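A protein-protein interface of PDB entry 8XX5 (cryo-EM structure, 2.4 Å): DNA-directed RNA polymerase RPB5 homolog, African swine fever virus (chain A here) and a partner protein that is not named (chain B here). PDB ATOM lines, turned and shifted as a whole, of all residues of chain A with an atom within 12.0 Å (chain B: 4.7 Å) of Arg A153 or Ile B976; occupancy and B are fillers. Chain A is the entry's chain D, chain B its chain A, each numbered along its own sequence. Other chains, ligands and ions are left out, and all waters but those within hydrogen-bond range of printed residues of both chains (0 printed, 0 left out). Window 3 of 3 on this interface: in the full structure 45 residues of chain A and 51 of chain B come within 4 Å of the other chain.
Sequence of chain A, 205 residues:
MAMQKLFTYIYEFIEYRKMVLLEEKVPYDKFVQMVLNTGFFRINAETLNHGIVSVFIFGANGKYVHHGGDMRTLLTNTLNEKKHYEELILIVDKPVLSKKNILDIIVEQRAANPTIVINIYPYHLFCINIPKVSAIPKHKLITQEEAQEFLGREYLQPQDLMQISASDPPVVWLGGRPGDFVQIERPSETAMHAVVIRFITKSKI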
ATOM      1  N   ILE A 142      20.961  19.982 -27.133  1.00  0.00           N
ATOM      2  CA  ILE A 142      22.091  19.945 -26.216  1.00  0.00           C
ATOM      3  C   ILE A 142      23.373  20.031 -27.029  1.00  0.00           C
ATOM      4  O   ILE A 142      23.467  19.459 -28.122  1.00  0.00           O
ATOM      5  CB  ILE A 142      22.079  18.681 -25.336  1.00  0.00           C
ATOM      6  CG1 ILE A 142      21.851  17.433 -26.186  1.00  0.00           C
ATOM      7  CG2 ILE A 142      21.014  18.796 -24.260  1.00  0.00           C
ATOM      8  CD1 ILE A 142      22.278  16.157 -25.507  1.00  0.00           C
ATOM      9  N   GLN A 144      27.288  19.604 -28.312  1.00  0.00           N
ATOM     10  CA  GLN A 144      28.012  18.375 -28.612  1.00  0.00           C
ATOM     11  C   GLN A 144      28.859  17.912 -27.435  1.00  0.00           C
ATOM     12  O   GLN A 144      29.113  16.714 -27.293  1.00  0.00           O
ATOM     13  CB  GLN A 144      28.885  18.569 -29.853  1.00  0.00           C
ATOM     14  CG  GLN A 144      28.312  17.964 -31.128  1.00  0.00           C
ATOM     15  CD  GLN A 144      28.440  16.449 -31.188  1.00  0.00           C
ATOM     16  OE1 GLN A 144      28.656  15.785 -30.174  1.00  0.00           O
ATOM     17  NE2 GLN A 144      28.302  15.896 -32.386  1.00  0.00           N
ATOM     18  N   GLU A 145      29.299  18.836 -26.581  1.00  0.00           N
ATOM     19  CA  GLU A 145      30.101  18.450 -25.422  1.00  0.00           C
ATOM     20  C   GLU A 145      29.265  17.683 -24.403  1.00  0.00           C
ATOM     21  O   GLU A 145      29.698  16.647 -23.879  1.00  0.00           O
ATOM     22  CB  GLU A 145      30.729  19.690 -24.788  1.00  0.00           C
ATOM     23  CG  GLU A 145      31.369  20.640 -25.789  1.00  0.00           C
ATOM     24  CD  GLU A 145      30.440  21.767 -26.208  1.00  0.00           C
ATOM     25  OE1 GLU A 145      29.968  22.512 -25.324  1.00  0.00           O
ATOM     26  OE2 GLU A 145      30.184  21.907 -27.422  1.00  0.00           O
ATOM     27  N   GLU A 146      28.061  18.180 -24.107  1.00  0.00           N
ATOM     28  CA  GLU A 146      27.173  17.474 -23.189  1.00  0.00           C
ATOM     29  C   GLU A 146      26.784  16.112 -23.743  1.00  0.00           C
ATOM     30  O   GLU A 146      26.746  15.118 -23.008  1.00  0.00           O
ATOM     31  CB  GLU A 146      25.925  18.313 -22.914  1.00  0.00           C
ATOM     32  CG  GLU A 146      26.189  19.799 -22.767  1.00  0.00           C
ATOM     33  CD  GLU A 146      24.978  20.555 -22.261  1.00  0.00           C
ATOM     34  OE1 GLU A 146      24.756  20.572 -21.032  1.00  0.00           O
ATOM     35  OE2 GLU A 146      24.246  21.135 -23.092  1.00  0.00           O
ATOM     36  N   ALA A 147      26.489  16.048 -25.042  1.00  0.00           N
ATOM     37  CA  ALA A 147      26.157  14.770 -25.659  1.00  0.00           C
ATOM     38  C   ALA A 147      27.334  13.808 -25.600  1.00  0.00           C
ATOM     39  O   ALA A 147      27.155  12.614 -25.339  1.00  0.00           O
ATOM     40  CB  ALA A 147      25.712  14.987 -27.102  1.00  0.00           C
ATOM     41  N   GLN A 148      28.548  14.307 -25.841  1.00  0.00           N
ATOM     42  CA  GLN A 148      29.726  13.449 -25.790  1.00  0.00           C
ATOM     43  C   GLN A 148      29.964  12.914 -24.385  1.00  0.00           C
ATOM     44  O   GLN A 148      30.297  11.738 -24.218  1.00  0.00           O
ATOM     45  CB  GLN A 148      30.954  14.204 -26.294  1.00  0.00           C
ATOM     46  CG  GLN A 148      31.069  14.264 -27.810  1.00  0.00           C
ATOM     47  CD  GLN A 148      30.728  12.944 -28.475  1.00  0.00           C
ATOM     48  OE1 GLN A 148      31.344  11.917 -28.193  1.00  0.00           O
ATOM     49  NE2 GLN A 148      29.741  12.966 -29.363  1.00  0.00           N
ATOM     50  N   GLU A 149      29.802  13.754 -23.360  1.00  0.00           N
ATOM     51  CA  GLU A 149      30.001  13.264 -21.999  1.00  0.00           C
ATOM     52  C   GLU A 149      28.908  12.276 -21.602  1.00  0.00           C
ATOM     53  O   GLU A 149      29.181  11.278 -20.920  1.00  0.00           O
ATOM     54  CB  GLU A 149      30.086  14.435 -21.012  1.00  0.00           C
ATOM     55  CG  GLU A 149      28.777  15.135 -20.698  1.00  0.00           C
ATOM     56  CD  GLU A 149      28.107  14.592 -19.451  1.00  0.00           C
ATOM     57  OE1 GLU A 149      28.770  13.855 -18.691  1.00  0.00           O
ATOM     58  OE2 GLU A 149      26.914  14.896 -19.237  1.00  0.00           O
ATOM     59  N   PHE A 150      27.668  12.520 -22.042  1.00  0.00           N
ATOM     60  CA  PHE A 150      26.590  11.574 -21.779  1.00  0.00           C
ATOM     61  C   PHE A 150      26.860  10.232 -22.447  1.00  0.00           C
ATOM     62  O   PHE A 150      26.648   9.175 -21.843  1.00  0.00           O
ATOM     63  CB  PHE A 150      25.259  12.159 -22.254  1.00  0.00           C
ATOM     64  CG  PHE A 150      24.162  11.144 -22.399  1.00  0.00           C
ATOM     65  CD1 PHE A 150      23.451  10.714 -21.293  1.00  0.00           C
ATOM     66  CD2 PHE A 150      23.833  10.629 -23.640  1.00  0.00           C
ATOM     67  CE1 PHE A 150      22.441   9.784 -21.422  1.00  0.00           C
ATOM     68  CE2 PHE A 150      22.825   9.698 -23.775  1.00  0.00           C
ATOM     69  CZ  PHE A 150      22.128   9.277 -22.664  1.00  0.00           C
ATOM     70  N   LEU A 151      27.330  10.254 -23.696  1.00  0.00           N
ATOM     71  CA  LEU A 151      27.626   9.014 -24.402  1.00  0.00           C
ATOM     72  C   LEU A 151      28.825   8.301 -23.793  1.00  0.00           C
ATOM     73  O   LEU A 151      28.866   7.067 -23.752  1.00  0.00           O
ATOM     74  CB  LEU A 151      27.868   9.300 -25.883  1.00  0.00           C
ATOM     75  CG  LEU A 151      26.653   9.737 -26.704  1.00  0.00           C
ATOM     76  CD1 LEU A 151      27.091  10.290 -28.046  1.00  0.00           C
ATOM     77  CD2 LEU A 151      25.681   8.586 -26.886  1.00  0.00           C
ATOM     78  N   GLY A 152      29.816   9.062 -23.325  1.00  0.00           N
ATOM     79  CA  GLY A 152      30.973   8.451 -22.696  1.00  0.00           C
ATOM     80  C   GLY A 152      30.633   7.771 -21.387  1.00  0.00           C
ATOM     81  O   GLY A 152      31.141   6.687 -21.092  1.00  0.00           O
ATOM     82  N   ARG A 153      29.776   8.399 -20.578  1.00  0.00           N
ATOM     83  CA  ARG A 153      29.343   7.751 -19.344  1.00  0.00           C
ATOM     84  C   ARG A 153      28.541   6.490 -19.638  1.00  0.00           C
ATOM     85  O   ARG A 153      28.679   5.480 -18.941  1.00  0.00           O
ATOM     86  CB  ARG A 153      28.521   8.718 -18.495  1.00  0.00           C
ATOM     87  CG  ARG A 153      28.309   8.236 -17.074  1.00  0.00           C
ATOM     88  CD  ARG A 153      26.838   8.171 -16.722  1.00  0.00           C
ATOM     89  NE  ARG A 153      26.601   7.361 -15.532  1.00  0.00           N
ATOM     90  CZ  ARG A 153      25.668   6.424 -15.438  1.00  0.00           C
ATOM     91  NH1 ARG A 153      24.851   6.160 -16.442  1.00  0.00           N
ATOM     92  NH2 ARG A 153      25.551   5.739 -14.305  1.00  0.00           N
ATOM     93  N   GLU A 154      27.699   6.530 -20.668  1.00  0.00           N
ATOM     94  CA  GLU A 154      26.827   5.413 -21.002  1.00  0.00           C
ATOM     95  C   GLU A 154      27.500   4.365 -21.879  1.00  0.00           C
ATOM     96  O   GLU A 154      26.872   3.343 -22.173  1.00  0.00           O
ATOM     97  CB  GLU A 154      25.565   5.925 -21.700  1.00  0.00           C
ATOM     98  CG  GLU A 154      24.714   6.847 -20.846  1.00  0.00           C
ATOM     99  CD  GLU A 154      23.875   6.094 -19.837  1.00  0.00           C
ATOM    100  OE1 GLU A 154      23.255   5.079 -20.215  1.00  0.00           O
ATOM    101  OE2 GLU A 154      23.839   6.515 -18.661  1.00  0.00           O
ATOM    102  N   TYR A 155      28.748   4.590 -22.296  1.00  0.00           N
ATOM    103  CA  TYR A 155      29.456   3.689 -23.208  1.00  0.00           C
ATOM    104  C   TYR A 155      28.656   3.475 -24.493  1.00  0.00           C
ATOM    105  O   TYR A 155      28.462   2.349 -24.952  1.00  0.00           O
ATOM    106  CB  TYR A 155      29.777   2.355 -22.529  1.00  0.00           C
ATOM    107  CG  TYR A 155      31.116   2.325 -21.832  1.00  0.00           C
ATOM    108  CD1 TYR A 155      32.287   2.582 -22.528  1.00  0.00           C
ATOM    109  CD2 TYR A 155      31.208   2.047 -20.477  1.00  0.00           C
ATOM    110  CE1 TYR A 155      33.512   2.559 -21.896  1.00  0.00           C
ATOM    111  CE2 TYR A 155      32.429   2.019 -19.835  1.00  0.00           C
ATOM    112  CZ  TYR A 155      33.577   2.277 -20.550  1.00  0.00           C
ATOM    113  OH  TYR A 155      34.797   2.252 -19.915  1.00  0.00           O
ATOM    114  N   LEU A 156      28.187   4.576 -25.072  1.00  0.00           N
ATOM    115  CA  LEU A 156      27.300   4.538 -26.223  1.00  0.00           C
ATOM    116  C   LEU A 156      27.872   5.360 -27.370  1.00  0.00           C
ATOM    117  O   LEU A 156      28.634   6.309 -27.170  1.00  0.00           O
ATOM    118  CB  LEU A 156      25.907   5.069 -25.866  1.00  0.00           C
ATOM    119  CG  LEU A 156      24.944   4.152 -25.116  1.00  0.00           C
ATOM    120  CD1 LEU A 156      23.657   4.895 -24.827  1.00  0.00           C
ATOM    121  CD2 LEU A 156      24.668   2.885 -25.902  1.00  0.00           C
ATOM    122  N   GLN A 157      27.489   4.978 -28.576  1.00  0.00           N
ATOM    123  CA  GLN A 157      27.721   5.735 -29.794  1.00  0.00           C
ATOM    124  C   GLN A 157      26.496   6.562 -30.143  1.00  0.00           C
ATOM    125  O   GLN A 157      25.381   6.252 -29.713  1.00  0.00           O
ATOM    126  CB  GLN A 157      28.060   4.793 -30.955  1.00  0.00           C
ATOM    127  CG  GLN A 157      28.768   3.522 -30.544  1.00  0.00           C
ATOM    128  CD  GLN A 157      30.202   3.782 -30.135  1.00  0.00           C
ATOM    129  OE1 GLN A 157      30.654   3.315 -29.090  1.00  0.00           O
ATOM    130  NE2 GLN A 157      30.929   4.522 -30.959  1.00  0.00           N
ATOM    131  N   PRO A 158      26.666   7.637 -30.915  1.00  0.00           N
ATOM    132  CA  PRO A 158      25.496   8.420 -31.342  1.00  0.00           C
ATOM    133  C   PRO A 158      24.500   7.619 -32.159  1.00  0.00           C
ATOM    134  O   PRO A 158      23.315   7.972 -32.183  1.00  0.00           O
ATOM    135  CB  PRO A 158      26.115   9.554 -32.169  1.00  0.00           C
ATOM    136  CG  PRO A 158      27.515   9.655 -31.681  1.00  0.00           C
ATOM    137  CD  PRO A 158      27.929   8.259 -31.343  1.00  0.00           C
ATOM    138  N   ASP A 160      23.588   4.545 -31.534  1.00  0.00           N
ATOM    139  CA  ASP A 160      22.812   3.674 -30.664  1.00  0.00           C
ATOM    140  C   ASP A 160      21.604   4.376 -30.064  1.00  0.00           C
ATOM    141  O   ASP A 160      20.706   3.704 -29.546  1.00  0.00           O
ATOM    142  CB  ASP A 160      23.695   3.132 -29.539  1.00  0.00           C
ATOM    143  CG  ASP A 160      24.754   2.173 -30.041  1.00  0.00           C
ATOM    144  OD1 ASP A 160      24.570   1.601 -31.136  1.00  0.00           O
ATOM    145  OD2 ASP A 160      25.771   1.992 -29.340  1.00  0.00           O
ATOM    146  N   LEU A 161      21.560   5.702 -30.126  1.00  0.00           N
ATOM    147  CA  LEU A 161      20.464   6.455 -29.543  1.00  0.00           C
ATOM    148  C   LEU A 161      19.200   6.311 -30.381  1.00  0.00           C
ATOM    149  O   LEU A 161      19.238   5.958 -31.563  1.00  0.00           O
ATOM    150  CB  LEU A 161      20.835   7.931 -29.422  1.00  0.00           C
ATOM    151  CG  LEU A 161      21.845   8.302 -28.341  1.00  0.00           C
ATOM    152  CD1 LEU A 161      21.933   9.807 -28.212  1.00  0.00           C
ATOM    153  CD2 LEU A 161      21.464   7.670 -27.015  1.00  0.00           C
ATOM    154  N   PHE A 181      21.965  16.466 -31.278  1.00  0.00           N
ATOM    155  CA  PHE A 181      21.276  15.757 -30.211  1.00  0.00           C
ATOM    156  C   PHE A 181      20.214  16.658 -29.604  1.00  0.00           C
ATOM    157  O   PHE A 181      20.450  17.848 -29.379  1.00  0.00           O
ATOM    158  CB  PHE A 181      22.256  15.303 -29.128  1.00  0.00           C
ATOM    159  CG  PHE A 181      23.306  14.353 -29.620  1.00  0.00           C
ATOM    160  CD1 PHE A 181      24.433  14.820 -30.274  1.00  0.00           C
ATOM    161  CD2 PHE A 181      23.171  12.991 -29.421  1.00  0.00           C
ATOM    162  CE1 PHE A 181      25.401  13.948 -30.720  1.00  0.00           C
ATOM    163  CE2 PHE A 181      24.136  12.116 -29.867  1.00  0.00           C
ATOM    164  CZ  PHE A 181      25.252  12.596 -30.517  1.00  0.00           C
ATOM    165  N   VAL A 195      13.557  12.125 -18.910  1.00  0.00           N
ATOM    166  CA  VAL A 195      14.476  12.790 -19.824  1.00  0.00           C
ATOM    167  C   VAL A 195      15.011  11.758 -20.805  1.00  0.00           C
ATOM    168  O   VAL A 195      15.462  10.682 -20.399  1.00  0.00           O
ATOM    169  CB  VAL A 195      15.626  13.484 -19.070  1.00  0.00           C
ATOM    170  CG1 VAL A 195      16.850  13.609 -19.956  1.00  0.00           C
ATOM    171  CG2 VAL A 195      15.181  14.850 -18.586  1.00  0.00           C
ATOM    172  N   ILE A 197      17.324  11.495 -24.646  1.00  0.00           N
ATOM    173  CA  ILE A 197      18.178  12.163 -25.619  1.00  0.00           C
ATOM    174  C   ILE A 197      18.075  11.402 -26.931  1.00  0.00           C
ATOM    175  O   ILE A 197      18.312  10.189 -26.970  1.00  0.00           O
ATOM    176  CB  ILE A 197      19.636  12.248 -25.142  1.00  0.00           C
ATOM    177  CG1 ILE A 197      19.747  13.211 -23.958  1.00  0.00           C
ATOM    178  CG2 ILE A 197      20.543  12.688 -26.276  1.00  0.00           C
ATOM    179  CD1 ILE A 197      21.130  13.295 -23.368  1.00  0.00           C
ATOM    180  N   TYR B 841      22.937  -0.857 -17.630  1.00  0.00           N
ATOM    181  CA  TYR B 841      22.505   0.477 -17.250  1.00  0.00           C
ATOM    182  C   TYR B 841      21.014   0.529 -16.966  1.00  0.00           C
ATOM    183  O   TYR B 841      20.475   1.614 -16.729  1.00  0.00           O
ATOM    184  CB  TYR B 841      22.858   1.484 -18.345  1.00  0.00           C
ATOM    185  CG  TYR B 841      24.335   1.765 -18.487  1.00  0.00           C
ATOM    186  CD1 TYR B 841      25.185   0.840 -19.079  1.00  0.00           C
ATOM    187  CD2 TYR B 841      24.878   2.959 -18.042  1.00  0.00           C
ATOM    188  CE1 TYR B 841      26.531   1.095 -19.213  1.00  0.00           C
ATOM    189  CE2 TYR B 841      26.223   3.224 -18.176  1.00  0.00           C
ATOM    190  CZ  TYR B 841      27.046   2.288 -18.760  1.00  0.00           C
ATOM    191  OH  TYR B 841      28.390   2.546 -18.892  1.00  0.00           O
ATOM    192  N   PRO B 972      18.959   8.927  -6.328  1.00  0.00           N
ATOM    193  CA  PRO B 972      19.226   8.339  -7.650  1.00  0.00           C
ATOM    194  C   PRO B 972      20.435   7.414  -7.688  1.00  0.00           C
ATOM    195  O   PRO B 972      20.693   6.779  -8.714  1.00  0.00           O
ATOM    196  CB  PRO B 972      19.447   9.569  -8.540  1.00  0.00           C
ATOM    197  CG  PRO B 972      18.774  10.675  -7.837  1.00  0.00           C
ATOM    198  CD  PRO B 972      18.976  10.399  -6.389  1.00  0.00           C
ATOM    199  N   TYR B 973      21.182   7.327  -6.589  1.00  0.00           N
ATOM    200  CA  TYR B 973      22.320   6.418  -6.526  1.00  0.00           C
ATOM    201  C   TYR B 973      21.912   4.967  -6.326  1.00  0.00           C
ATOM    202  O   TYR B 973      22.764   4.084  -6.459  1.00  0.00           O
ATOM    203  CB  TYR B 973      23.276   6.838  -5.412  1.00  0.00           C
ATOM    204  CG  TYR B 973      24.200   7.962  -5.804  1.00  0.00           C
ATOM    205  CD1 TYR B 973      25.042   7.841  -6.899  1.00  0.00           C
ATOM    206  CD2 TYR B 973      24.229   9.144  -5.083  1.00  0.00           C
ATOM    207  CE1 TYR B 973      25.886   8.867  -7.263  1.00  0.00           C
ATOM    208  CE2 TYR B 973      25.070  10.174  -5.441  1.00  0.00           C
ATOM    209  CZ  TYR B 973      25.896  10.029  -6.530  1.00  0.00           C
ATOM    210  OH  TYR B 973      26.734  11.054  -6.888  1.00  0.00           O
ATOM    211  N   VAL B 974      20.645   4.695  -6.007  1.00  0.00           N
ATOM    212  CA  VAL B 974      20.186   3.312  -5.995  1.00  0.00           C
ATOM    213  C   VAL B 974      20.187   2.736  -7.401  1.00  0.00           C
ATOM    214  O   VAL B 974      20.206   1.512  -7.569  1.00  0.00           O
ATOM    215  CB  VAL B 974      18.790   3.189  -5.352  1.00  0.00           C
ATOM    216  CG1 VAL B 974      18.754   3.913  -4.017  1.00  0.00           C
ATOM    217  CG2 VAL B 974      17.713   3.715  -6.286  1.00  0.00           C
ATOM    218  N   PHE B 975      20.170   3.593  -8.420  1.00  0.00           N
ATOM    219  CA  PHE B 975      20.263   3.150  -9.801  1.00  0.00           C
ATOM    220  C   PHE B 975      21.692   2.871 -10.242  1.00  0.00           C
ATOM    221  O   PHE B 975      21.881   2.338 -11.340  1.00  0.00           O
ATOM    222  CB  PHE B 975      19.646   4.194 -10.736  1.00  0.00           C
ATOM    223  CG  PHE B 975      18.166   4.365 -10.566  1.00  0.00           C
ATOM    224  CD1 PHE B 975      17.290   3.380 -10.982  1.00  0.00           C
ATOM    225  CD2 PHE B 975      17.649   5.517  -9.999  1.00  0.00           C
ATOM    226  CE1 PHE B 975      15.928   3.535 -10.829  1.00  0.00           C
ATOM    227  CE2 PHE B 975      16.288   5.678  -9.845  1.00  0.00           C
ATOM    228  CZ  PHE B 975      15.428   4.686 -10.260  1.00  0.00           C
ATOM    229  N   ILE B 976      22.701   3.212  -9.438  1.00  0.00           N
ATOM    230  CA  ILE B 976      24.070   2.987  -9.882  1.00  0.00           C
ATOM    231  C   ILE B 976      24.783   1.982  -8.984  1.00  0.00           C
ATOM    232  O   ILE B 976      24.933   0.815  -9.358  1.00  0.00           O
ATOM    233  CB  ILE B 976      24.838   4.322  -9.918  1.00  0.00           C
ATOM    234  CG1 ILE B 976      23.933   5.440 -10.437  1.00  0.00           C
ATOM    235  CG2 ILE B 976      26.089   4.202 -10.763  1.00  0.00           C
ATOM    236  CD1 ILE B 976      24.594   6.790 -10.498  1.00  0.00           C
ATOM    237  N   ASN B 977      25.164   2.409  -7.776  1.00  0.00           N
ATOM    238  CA  ASN B 977      25.761   1.543  -6.760  1.00  0.00           C
ATOM    239  C   ASN B 977      26.139   2.351  -5.525  1.00  0.00           C
ATOM    240  O   ASN B 977      26.006   3.579  -5.512  1.00  0.00           O
ATOM    241  CB  ASN B 977      26.992   0.784  -7.280  1.00  0.00           C
ATOM    242  CG  ASN B 977      28.043   1.689  -7.881  1.00  0.00           C
ATOM    243  OD1 ASN B 977      28.315   2.772  -7.374  1.00  0.00           O
ATOM    244  ND2 ASN B 977      28.659   1.233  -8.959  1.00  0.00           N
ATOM    245  N   GLN B 980      29.603   4.710  -6.321  1.00  0.00           N
ATOM    246  CA  GLN B 980      29.429   6.046  -6.879  1.00  0.00           C
ATOM    247  C   GLN B 980      28.753   6.980  -5.888  1.00  0.00           C
ATOM    248  O   GLN B 980      29.022   8.186  -5.894  1.00  0.00           O
ATOM    249  CB  GLN B 980      28.631   5.976  -8.181  1.00  0.00           C
ATOM    250  CG  GLN B 980      29.247   5.088  -9.252  1.00  0.00           C
ATOM    251  CD  GLN B 980      30.735   5.309  -9.425  1.00  0.00           C
ATOM    252  OE1 GLN B 980      31.189   6.434  -9.627  1.00  0.00           O
ATOM    253  NE2 GLN B 980      31.504   4.232  -9.347  1.00  0.00           N
ATOM    254  N   PRO B 988      23.467  11.184 -13.842  1.00  0.00           N
ATOM    255  CA  PRO B 988      22.863  11.589 -15.115  1.00  0.00           C
ATOM    256  C   PRO B 988      21.477  12.180 -14.899  1.00  0.00           C
ATOM    257  O   PRO B 988      20.778  11.844 -13.942  1.00  0.00           O
ATOM    258  CB  PRO B 988      22.797  10.282 -15.913  1.00  0.00           C
ATOM    259  CG  PRO B 988      23.745   9.358 -15.235  1.00  0.00           C
ATOM    260  CD  PRO B 988      23.752   9.742 -13.796  1.00  0.00           C
ATOM    261  N   TYR B 990      18.668  11.840 -16.525  1.00  0.00           N
ATOM    262  CA  TYR B 990      17.548  10.909 -16.588  1.00  0.00           C
ATOM    263  C   TYR B 990      17.424  10.087 -15.310  1.00  0.00           C
ATOM    264  O   TYR B 990      16.308   9.754 -14.897  1.00  0.00           O
ATOM    265  CB  TYR B 990      17.678  10.007 -17.817  1.00  0.00           C
ATOM    266  CG  TYR B 990      18.712   8.908 -17.715  1.00  0.00           C
ATOM    267  CD1 TYR B 990      20.038   9.144 -18.043  1.00  0.00           C
ATOM    268  CD2 TYR B 990      18.356   7.629 -17.314  1.00  0.00           C
ATOM    269  CE1 TYR B 990      20.981   8.144 -17.960  1.00  0.00           C
ATOM    270  CE2 TYR B 990      19.293   6.623 -17.229  1.00  0.00           C
ATOM    271  CZ  TYR B 990      20.603   6.886 -17.552  1.00  0.00           C
ATOM    272  OH  TYR B 990      21.540   5.882 -17.468  1.00  0.00           O
ATOM    273  N   LEU B 991      18.545   9.768 -14.662  1.00  0.00           N
ATOM    274  CA  LEU B 991      18.475   9.074 -13.380  1.00  0.00           C
ATOM    275  C   LEU B 991      17.950   9.987 -12.279  1.00  0.00           C
ATOM    276  O   LEU B 991      17.282   9.515 -11.352  1.00  0.00           O
ATOM    277  CB  LEU B 991      19.844   8.515 -13.005  1.00  0.00           C
ATOM    278  CG  LEU B 991      20.249   7.234 -13.733  1.00  0.00           C
ATOM    279  CD1 LEU B 991      21.483   6.627 -13.097  1.00  0.00           C
ATOM    280  CD2 LEU B 991      19.102   6.240 -13.736  1.00  0.00           C
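Glu A149 touches none of the printed residues of chain B.
Of chain B, only Tyr B841 (2.9 Å), Ile B976 (3.9 Å), Pro B988 (3.5 Å) and Tyr B990 (3.5 Å) come within 4 Å of Arg A153.
Printed residues of chain B within 4 Å of Glu A154: Tyr B841 (3.4 Å) and Tyr B990 (2.7 Å).
Of the printed residues of chain B, Tyr A155 touches Tyr B841.
Leu A156 touches none of the printed residues of chain B.
Printed residues of chain B within 4 Å of Val A195: Tyr B990 (3.5 Å).
Tyr B841 touches just these residues of chain A: Arg A153, Glu A154 and Tyr A155.
No residue of chain A comes within 4 Å of Pro B972.
No residue of chain A comes within 4 Å of Phe B975.
Of the printed residues of chain A, Ile B976 touches Arg A153.
No residue of chain A comes within 4 Å of Asn B977.
No residue of chain A comes within 4 Å of Gln B980.
Printed residues of chain A within 4 Å of Pro B988: Arg A153.
Of the printed residues of chain A, Tyr B990 touches Arg A153, Glu A154 and Val A195.
The nearest residue of chain B that does not touch Arg A153 is Leu B991 (4.3 Å).
Hydrophobic or aromatic side chains of chain B within 4 Å of the printed part of chain A: Tyr B841, Ile B976, Pro B988 and Tyr B990.
Of the 21 printed residues of chain A, 4 touch a printed residue of chain B.
Hydrophobic or aromatic side chains of chain A that line the printed part of chain B: Tyr A155.
Among the printed residues, 8 pairs touch across the chains.
Among the printed residues, no Asp or Glu carboxylate lies within 4 Å of a Lys or Arg side-chain nitrogen of the other chain.
The side-chain hydroxyl of Tyr B841 sits at hydrogen-bond distance from the backbone carbonyl oxygen of Arg A153 (2.9 Å).
The side-chain hydroxyl (OH) of Tyr B990 is in hydrogen-bond range of the guanidinium group (NH1) of Arg A153 (3.5 Å).
The side-chain carboxylate (OE2) of Glu A154 is in hydrogen-bond range of the side-chain hydroxyl (OH) of Tyr B990 (2.7 Å).
NH1 of Arg A153 lies within salt-bridge range of OE2 of Glu A154 (2.5 Å).
Among the printed residues, pairs that only touch across the chains: Arg A153 with Ile B976, Arg A153 with Pro B988, Glu A154 with Tyr B841, Tyr A155 with Tyr B841 and Val A195 with Tyr B990.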
